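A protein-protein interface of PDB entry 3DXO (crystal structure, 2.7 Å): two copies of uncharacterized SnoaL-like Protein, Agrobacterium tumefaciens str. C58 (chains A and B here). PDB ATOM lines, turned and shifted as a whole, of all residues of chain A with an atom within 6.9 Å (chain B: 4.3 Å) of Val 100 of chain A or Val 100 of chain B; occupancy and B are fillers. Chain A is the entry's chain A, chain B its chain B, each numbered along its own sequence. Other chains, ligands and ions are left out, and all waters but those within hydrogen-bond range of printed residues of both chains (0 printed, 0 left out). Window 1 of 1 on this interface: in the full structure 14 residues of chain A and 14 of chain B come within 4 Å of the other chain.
Phe 79 of chain A touches Val 113 of chain B, and with the chains exchanged Val 113 of chain A touches Phe 79 of chain B.
Val 100 of chain A touches its own counterpart, Val 100 of chain B.
Val 100 of chain A touches Phe 115 of chain B, and with the chains exchanged Phe 115 of chain A touches Val 100 of chain B.
Positions printed for both chains: 79, 80, 99, 100, 101, 111, 112, 113 and 115.
Of the printed residues of chain B, Phe 79 of chain A touches Val 113 (3.8 Å).
Of chain B, only Val 100 and Phe 115 come within 4 Å of Val 100 of chain A.
Of the printed residues of chain B, Val 113 of chain A touches Phe 79 (3.8 Å).
Val 100 of chain B touches just these residues of chain A: Val 100 and Phe 115.
Printed residues of chain A within 4 Å of Val 113 of chain B: Phe 79 (3.8 Å).
The nearest printed residue of chain B that does not touch Val 100 of chain A is Val 113 of chain B (4.6 Å).
The nearest residue of chain A that does not touch Val 100 of chain B is Val 113 of chain A (4.6 Å).
Hydrophobic or aromatic side chains of chain A that line the printed part of chain B: Phe 79, Val 100, Val 113 and Phe 115.
Of the 9 printed residues of chain B, 4 touch a printed residue of chain A.
Printed residues of chain B that touch a printed residue of chain A: Phe 79, Val 100, Val 113 and Phe 115.
Among the printed residues, no Asp or Glu carboxylate lies within 4 Å of a Lys or Arg side-chain nitrogen of the other chain.
N of Val 100 of chain A sits at hydrogen-bond distance from O of Val 113 of chain A (3.0 Å).
The backbone carbonyl oxygen (O) of Val 100 of chain B lies within hydrogen-bond range of the backbone NH (N) of Val 113 of chain B, at 3.0 Å.
The backbone carbonyl oxygen (O) of Thr 98 of chain A lies within hydrogen-bond range of the backbone NH (N) of Phe 115 of chain A (2.9 Å).
Among the printed residues, merely in contact across the chains: Arg 81 of chain A with Phe 115 of chain B (3.6 Å), Val 100 of chain A with Phe 115 of chain B (3.6 Å), Phe 115 of chain A with Val 100 of chain B (3.8 Å), Phe 79 of chain A with Val 113 of chain B (3.8 Å), Val 113 of chain A with Phe 79 of chain B (3.8 Å) and Val 100 of chain A with Val 100 of chain B (3.9 Å).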
ATOM      1  N   PHE A  79      -3.355   6.662  -3.763  1.00  0.00           N
ATOM      2  CA  PHE A  79      -3.273   5.806  -4.929  1.00  0.00           C
ATOM      3  C   PHE A  79      -2.225   4.704  -4.817  1.00  0.00           C
ATOM      4  O   PHE A  79      -1.086   4.942  -4.425  1.00  0.00           O
ATOM      5  CB  PHE A  79      -2.993   6.620  -6.193  1.00  0.00           C
ATOM      6  CG  PHE A  79      -4.108   7.516  -6.573  1.00  0.00           C
ATOM      7  CD1 PHE A  79      -5.260   6.990  -7.167  1.00  0.00           C
ATOM      8  CD2 PHE A  79      -4.021   8.883  -6.362  1.00  0.00           C
ATOM      9  CE1 PHE A  79      -6.312   7.813  -7.511  1.00  0.00           C
ATOM     10  CE2 PHE A  79      -5.066   9.713  -6.719  1.00  0.00           C
ATOM     11  CZ  PHE A  79      -6.209   9.188  -7.293  1.00  0.00           C
ATOM     12  N   THR A  80      -2.640   3.504  -5.209  1.00  0.00           N
ATOM     13  CA  THR A  80      -1.759   2.356  -5.326  1.00  0.00           C
ATOM     14  C   THR A  80      -1.891   1.779  -6.743  1.00  0.00           C
ATOM     15  O   THR A  80      -3.007   1.665  -7.279  1.00  0.00           O
ATOM     16  CB  THR A  80      -2.128   1.272  -4.302  1.00  0.00           C
ATOM     17  OG1 THR A  80      -1.954   1.818  -2.991  1.00  0.00           O
ATOM     18  CG2 THR A  80      -1.248   0.021  -4.483  1.00  0.00           C
ATOM     19  N   ARG A  81      -0.755   1.442  -7.345  1.00  0.00           N
ATOM     20  CA  ARG A  81      -0.729   0.786  -8.647  1.00  0.00           C
ATOM     21  C   ARG A  81      -0.012  -0.532  -8.532  1.00  0.00           C
ATOM     22  O   ARG A  81       1.022  -0.609  -7.880  1.00  0.00           O
ATOM     23  CB  ARG A  81       0.018   1.623  -9.674  1.00  0.00           C
ATOM     24  CG  ARG A  81       0.287   0.825 -10.968  1.00  0.00           C
ATOM     25  CD  ARG A  81       1.024   1.587 -12.034  1.00  0.00           C
ATOM     26  NE  ARG A  81       2.377   1.991 -11.639  1.00  0.00           N
ATOM     27  CZ  ARG A  81       3.322   2.339 -12.498  1.00  0.00           C
ATOM     28  NH1 ARG A  81       3.082   2.328 -13.791  1.00  0.00           N
ATOM     29  NH2 ARG A  81       4.505   2.682 -12.075  1.00  0.00           N
ATOM     30  N   PHE A  82      -0.544  -1.562  -9.177  1.00  0.00           N
ATOM     31  CA  PHE A  82       0.123  -2.870  -9.198  1.00  0.00           C
ATOM     32  C   PHE A  82      -0.325  -3.699 -10.396  1.00  0.00           C
ATOM     33  O   PHE A  82      -1.345  -3.432 -11.023  1.00  0.00           O
ATOM     34  CB  PHE A  82      -0.142  -3.651  -7.910  1.00  0.00           C
ATOM     35  CG  PHE A  82      -1.586  -3.926  -7.688  1.00  0.00           C
ATOM     36  CD1 PHE A  82      -2.179  -5.044  -8.229  1.00  0.00           C
ATOM     37  CD2 PHE A  82      -2.367  -3.023  -6.986  1.00  0.00           C
ATOM     38  CE1 PHE A  82      -3.545  -5.271  -8.052  1.00  0.00           C
ATOM     39  CE2 PHE A  82      -3.716  -3.233  -6.787  1.00  0.00           C
ATOM     40  CZ  PHE A  82      -4.310  -4.349  -7.310  1.00  0.00           C
ATOM     41  N   THR A  98      -3.271  -4.731 -14.956  1.00  0.00           N
ATOM     42  CA  THR A  98      -2.707  -3.681 -14.121  1.00  0.00           C
ATOM     43  C   THR A  98      -3.873  -2.899 -13.518  1.00  0.00           C
ATOM     44  O   THR A  98      -4.884  -2.681 -14.183  1.00  0.00           O
ATOM     45  CB  THR A  98      -1.770  -2.781 -14.941  1.00  0.00           C
ATOM     46  OG1 THR A  98      -0.698  -3.582 -15.442  1.00  0.00           O
ATOM     47  CG2 THR A  98      -1.184  -1.693 -14.101  1.00  0.00           C
ATOM     48  N   ASP A  99      -3.757  -2.499 -12.258  1.00  0.00           N
ATOM     49  CA  ASP A  99      -4.847  -1.760 -11.620  1.00  0.00           C
ATOM     50  C   ASP A  99      -4.384  -0.518 -10.919  1.00  0.00           C
ATOM     51  O   ASP A  99      -3.246  -0.427 -10.479  1.00  0.00           O
ATOM     52  CB  ASP A  99      -5.566  -2.636 -10.584  1.00  0.00           C
ATOM     53  CG  ASP A  99      -6.214  -3.853 -11.200  1.00  0.00           C
ATOM     54  OD1 ASP A  99      -7.379  -3.779 -11.610  1.00  0.00           O
ATOM     55  OD2 ASP A  99      -5.562  -4.896 -11.228  1.00  0.00           O
ATOM     56  N   VAL A 100      -5.273   0.455 -10.837  1.00  0.00           N
ATOM     57  CA  VAL A 100      -5.011   1.660 -10.074  1.00  0.00           C
ATOM     58  C   VAL A 100      -6.149   1.613  -9.075  1.00  0.00           C
ATOM     59  O   VAL A 100      -7.313   1.491  -9.484  1.00  0.00           O
ATOM     60  CB  VAL A 100      -5.051   2.950 -10.927  1.00  0.00           C
ATOM     61  CG1 VAL A 100      -4.922   4.168 -10.012  1.00  0.00           C
ATOM     62  CG2 VAL A 100      -3.954   2.955 -11.992  1.00  0.00           C
ATOM     63  N   VAL A 101      -5.804   1.630  -7.785  1.00  0.00           N
ATOM     64  CA  VAL A 101      -6.779   1.545  -6.670  1.00  0.00           C
ATOM     65  C   VAL A 101      -6.731   2.833  -5.806  1.00  0.00           C
ATOM     66  O   VAL A 101      -5.653   3.352  -5.551  1.00  0.00           O
ATOM     67  CB  VAL A 101      -6.449   0.331  -5.795  1.00  0.00           C
ATOM     68  CG1 VAL A 101      -7.355   0.282  -4.566  1.00  0.00           C
ATOM     69  CG2 VAL A 101      -6.567  -0.942  -6.595  1.00  0.00           C
ATOM     70  N   SER A 102      -7.885   3.335  -5.369  1.00  0.00           N
ATOM     71  CA  SER A 102      -7.943   4.546  -4.568  1.00  0.00           C
ATOM     72  C   SER A 102      -8.564   4.218  -3.235  1.00  0.00           C
ATOM     73  O   SER A 102      -9.582   3.530  -3.178  1.00  0.00           O
ATOM     74  CB  SER A 102      -8.856   5.592  -5.190  1.00  0.00           C
ATOM     75  OG  SER A 102      -8.655   5.736  -6.583  1.00  0.00           O
ATOM     76  N   ASN A 111     -12.393   3.075  -5.211  1.00  0.00           N
ATOM     77  CA  ASN A 111     -12.364   3.148  -6.661  1.00  0.00           C
ATOM     78  C   ASN A 111     -11.251   2.283  -7.254  1.00  0.00           C
ATOM     79  O   ASN A 111     -10.104   2.338  -6.778  1.00  0.00           O
ATOM     80  CB  ASN A 111     -12.127   4.610  -7.075  1.00  0.00           C
ATOM     81  CG  ASN A 111     -12.631   4.912  -8.448  1.00  0.00           C
ATOM     82  OD1 ASN A 111     -13.690   4.433  -8.850  1.00  0.00           O
ATOM     83  ND2 ASN A 111     -11.881   5.709  -9.182  1.00  0.00           N
ATOM     84  N   VAL A 112     -11.593   1.479  -8.260  1.00  0.00           N
ATOM     85  CA  VAL A 112     -10.607   0.682  -8.958  1.00  0.00           C
ATOM     86  C   VAL A 112     -10.824   0.761 -10.455  1.00  0.00           C
ATOM     87  O   VAL A 112     -11.945   0.656 -10.910  1.00  0.00           O
ATOM     88  CB  VAL A 112     -10.664  -0.779  -8.537  1.00  0.00           C
ATOM     89  CG1 VAL A 112      -9.661  -1.631  -9.384  1.00  0.00           C
ATOM     90  CG2 VAL A 112     -10.408  -0.892  -7.046  1.00  0.00           C
ATOM     91  N   VAL A 113      -9.756   0.985 -11.206  1.00  0.00           N
ATOM     92  CA  VAL A 113      -9.808   0.984 -12.675  1.00  0.00           C
ATOM     93  C   VAL A 113      -8.729  -0.017 -13.123  1.00  0.00           C
ATOM     94  O   VAL A 113      -7.541   0.158 -12.794  1.00  0.00           O
ATOM     95  CB  VAL A 113      -9.535   2.422 -13.297  1.00  0.00           C
ATOM     96  CG1 VAL A 113      -9.535   2.374 -14.845  1.00  0.00           C
ATOM     97  CG2 VAL A 113     -10.544   3.458 -12.776  1.00  0.00           C
ATOM     98  N   GLY A 114      -9.151  -1.075 -13.823  1.00  0.00           N
ATOM     99  CA  GLY A 114      -8.232  -2.102 -14.338  1.00  0.00           C
ATOM    100  C   GLY A 114      -7.973  -2.073 -15.840  1.00  0.00           C
ATOM    101  O   GLY A 114      -8.769  -1.536 -16.609  1.00  0.00           O
ATOM    102  N   PHE A 115      -6.847  -2.638 -16.252  1.00  0.00           N
ATOM    103  CA  PHE A 115      -6.499  -2.756 -17.647  1.00  0.00           C
ATOM    104  C   PHE A 115      -5.933  -4.156 -17.934  1.00  0.00           C
ATOM    105  O   PHE A 115      -5.524  -4.848 -17.006  1.00  0.00           O
ATOM    106  CB  PHE A 115      -5.484  -1.689 -18.010  1.00  0.00           C
ATOM    107  CG  PHE A 115      -5.988  -0.276 -17.802  1.00  0.00           C
ATOM    108  CD1 PHE A 115      -5.858   0.348 -16.557  1.00  0.00           C
ATOM    109  CD2 PHE A 115      -6.595   0.423 -18.831  1.00  0.00           C
ATOM    110  CE1 PHE A 115      -6.330   1.633 -16.355  1.00  0.00           C
ATOM    111  CE2 PHE A 115      -7.066   1.700 -18.629  1.00  0.00           C
ATOM    112  CZ  PHE A 115      -6.936   2.309 -17.398  1.00  0.00           C
ATOM    113  N   PHE B  79     -11.743   5.753 -20.471  1.00  0.00           N
ATOM    114  CA  PHE B  79     -10.375   5.626 -19.934  1.00  0.00           C
ATOM    115  C   PHE B  79      -9.345   5.262 -20.990  1.00  0.00           C
ATOM    116  O   PHE B  79      -9.570   4.376 -21.826  1.00  0.00           O
ATOM    117  CB  PHE B  79     -10.300   4.567 -18.825  1.00  0.00           C
ATOM    118  CG  PHE B  79     -11.034   4.952 -17.593  1.00  0.00           C
ATOM    119  CD1 PHE B  79     -10.506   5.907 -16.732  1.00  0.00           C
ATOM    120  CD2 PHE B  79     -12.251   4.374 -17.291  1.00  0.00           C
ATOM    121  CE1 PHE B  79     -11.184   6.280 -15.589  1.00  0.00           C
ATOM    122  CE2 PHE B  79     -12.928   4.738 -16.145  1.00  0.00           C
ATOM    123  CZ  PHE B  79     -12.390   5.698 -15.293  1.00  0.00           C
ATOM    124  N   THR B  80      -8.220   5.967 -20.933  1.00  0.00           N
ATOM    125  CA  THR B  80      -7.058   5.682 -21.750  1.00  0.00           C
ATOM    126  C   THR B  80      -5.844   5.483 -20.827  1.00  0.00           C
ATOM    127  O   THR B  80      -5.704   6.153 -19.819  1.00  0.00           O
ATOM    128  CB  THR B  80      -6.791   6.824 -22.739  1.00  0.00           C
ATOM    129  OG1 THR B  80      -7.914   6.938 -23.628  1.00  0.00           O
ATOM    130  CG2 THR B  80      -5.509   6.568 -23.533  1.00  0.00           C
ATOM    131  N   ASP B  99       0.324   6.840 -17.270  1.00  0.00           N
ATOM    132  CA  ASP B  99      -0.824   7.642 -16.875  1.00  0.00           C
ATOM    133  C   ASP B  99      -2.155   6.984 -17.205  1.00  0.00           C
ATOM    134  O   ASP B  99      -2.271   6.205 -18.168  1.00  0.00           O
ATOM    135  CB  ASP B  99      -0.831   8.985 -17.617  1.00  0.00           C
ATOM    136  CG  ASP B  99       0.400   9.813 -17.365  1.00  0.00           C
ATOM    137  OD1 ASP B  99       0.514  10.454 -16.291  1.00  0.00           O
ATOM    138  OD2 ASP B  99       1.223   9.872 -18.307  1.00  0.00           O
ATOM    139  N   VAL B 100      -3.163   7.335 -16.404  1.00  0.00           N
ATOM    140  CA  VAL B 100      -4.534   6.939 -16.662  1.00  0.00           C
ATOM    141  C   VAL B 100      -5.266   8.264 -16.846  1.00  0.00           C
ATOM    142  O   VAL B 100      -5.259   9.089 -15.951  1.00  0.00           O
ATOM    143  CB  VAL B 100      -5.119   6.090 -15.546  1.00  0.00           C
ATOM    144  CG1 VAL B 100      -6.589   5.725 -15.867  1.00  0.00           C
ATOM    145  CG2 VAL B 100      -4.282   4.843 -15.410  1.00  0.00           C
ATOM    146  N   VAL B 101      -5.866   8.449 -18.023  1.00  0.00           N
ATOM    147  CA  VAL B 101      -6.582   9.669 -18.385  1.00  0.00           C
ATOM    148  C   VAL B 101      -8.089   9.397 -18.544  1.00  0.00           C
ATOM    149  O   VAL B 101      -8.471   8.361 -19.057  1.00  0.00           O
ATOM    150  CB  VAL B 101      -6.004  10.218 -19.711  1.00  0.00           C
ATOM    151  CG1 VAL B 101      -6.759  11.452 -20.177  1.00  0.00           C
ATOM    152  CG2 VAL B 101      -4.543  10.527 -19.537  1.00  0.00           C
ATOM    153  N   ASN B 111      -9.645  14.149 -15.838  1.00  0.00           N
ATOM    154  CA  ASN B 111      -8.925  13.542 -14.731  1.00  0.00           C
ATOM    155  C   ASN B 111      -7.683  12.773 -15.175  1.00  0.00           C
ATOM    156  O   ASN B 111      -7.757  11.990 -16.111  1.00  0.00           O
ATOM    157  CB  ASN B 111      -9.870  12.593 -13.979  1.00  0.00           C
ATOM    158  CG  ASN B 111      -9.490  12.433 -12.509  1.00  0.00           C
ATOM    159  OD1 ASN B 111      -9.029  13.392 -11.876  1.00  0.00           O
ATOM    160  ND2 ASN B 111      -9.692  11.235 -11.955  1.00  0.00           N
ATOM    161  N   VAL B 112      -6.540  13.024 -14.544  1.00  0.00           N
ATOM    162  CA  VAL B 112      -5.325  12.285 -14.879  1.00  0.00           C
ATOM    163  C   VAL B 112      -4.568  11.864 -13.630  1.00  0.00           C
ATOM    164  O   VAL B 112      -4.349  12.667 -12.728  1.00  0.00           O
ATOM    165  CB  VAL B 112      -4.370  13.087 -15.749  1.00  0.00           C
ATOM    166  CG1 VAL B 112      -3.054  12.305 -15.915  1.00  0.00           C
ATOM    167  CG2 VAL B 112      -5.016  13.393 -17.117  1.00  0.00           C
ATOM    168  N   VAL B 113      -4.185  10.599 -13.574  1.00  0.00           N
ATOM    169  CA  VAL B 113      -3.423  10.103 -12.458  1.00  0.00           C
ATOM    170  C   VAL B 113      -2.152   9.468 -13.029  1.00  0.00           C
ATOM    171  O   VAL B 113      -2.225   8.475 -13.730  1.00  0.00           O
ATOM    172  CB  VAL B 113      -4.234   9.087 -11.593  1.00  0.00           C
ATOM    173  CG1 VAL B 113      -3.371   8.507 -10.484  1.00  0.00           C
ATOM    174  CG2 VAL B 113      -5.480   9.743 -10.998  1.00  0.00           C
ATOM    175  N   PHE B 115       2.002   7.922 -12.665  1.00  0.00           N
ATOM    176  CA  PHE B 115       2.923   7.132 -11.832  1.00  0.00           C
ATOM    177  C   PHE B 115       4.332   7.136 -12.470  1.00  0.00           C
ATOM    178  O   PHE B 115       4.466   7.352 -13.648  1.00  0.00           O
ATOM    179  CB  PHE B 115       2.417   5.700 -11.698  1.00  0.00           C
ATOM    180  CG  PHE B 115       1.051   5.585 -11.079  1.00  0.00           C
ATOM    181  CD1 PHE B 115      -0.098   5.648 -11.864  1.00  0.00           C
ATOM    182  CD2 PHE B 115       0.915   5.404  -9.708  1.00  0.00           C
ATOM    183  CE1 PHE B 115      -1.362   5.550 -11.294  1.00  0.00           C
ATOM    184  CE2 PHE B 115      -0.338   5.284  -9.129  1.00  0.00           C
ATOM    185  CZ  PHE B 115      -1.492   5.353  -9.929  1.00  0.00           C
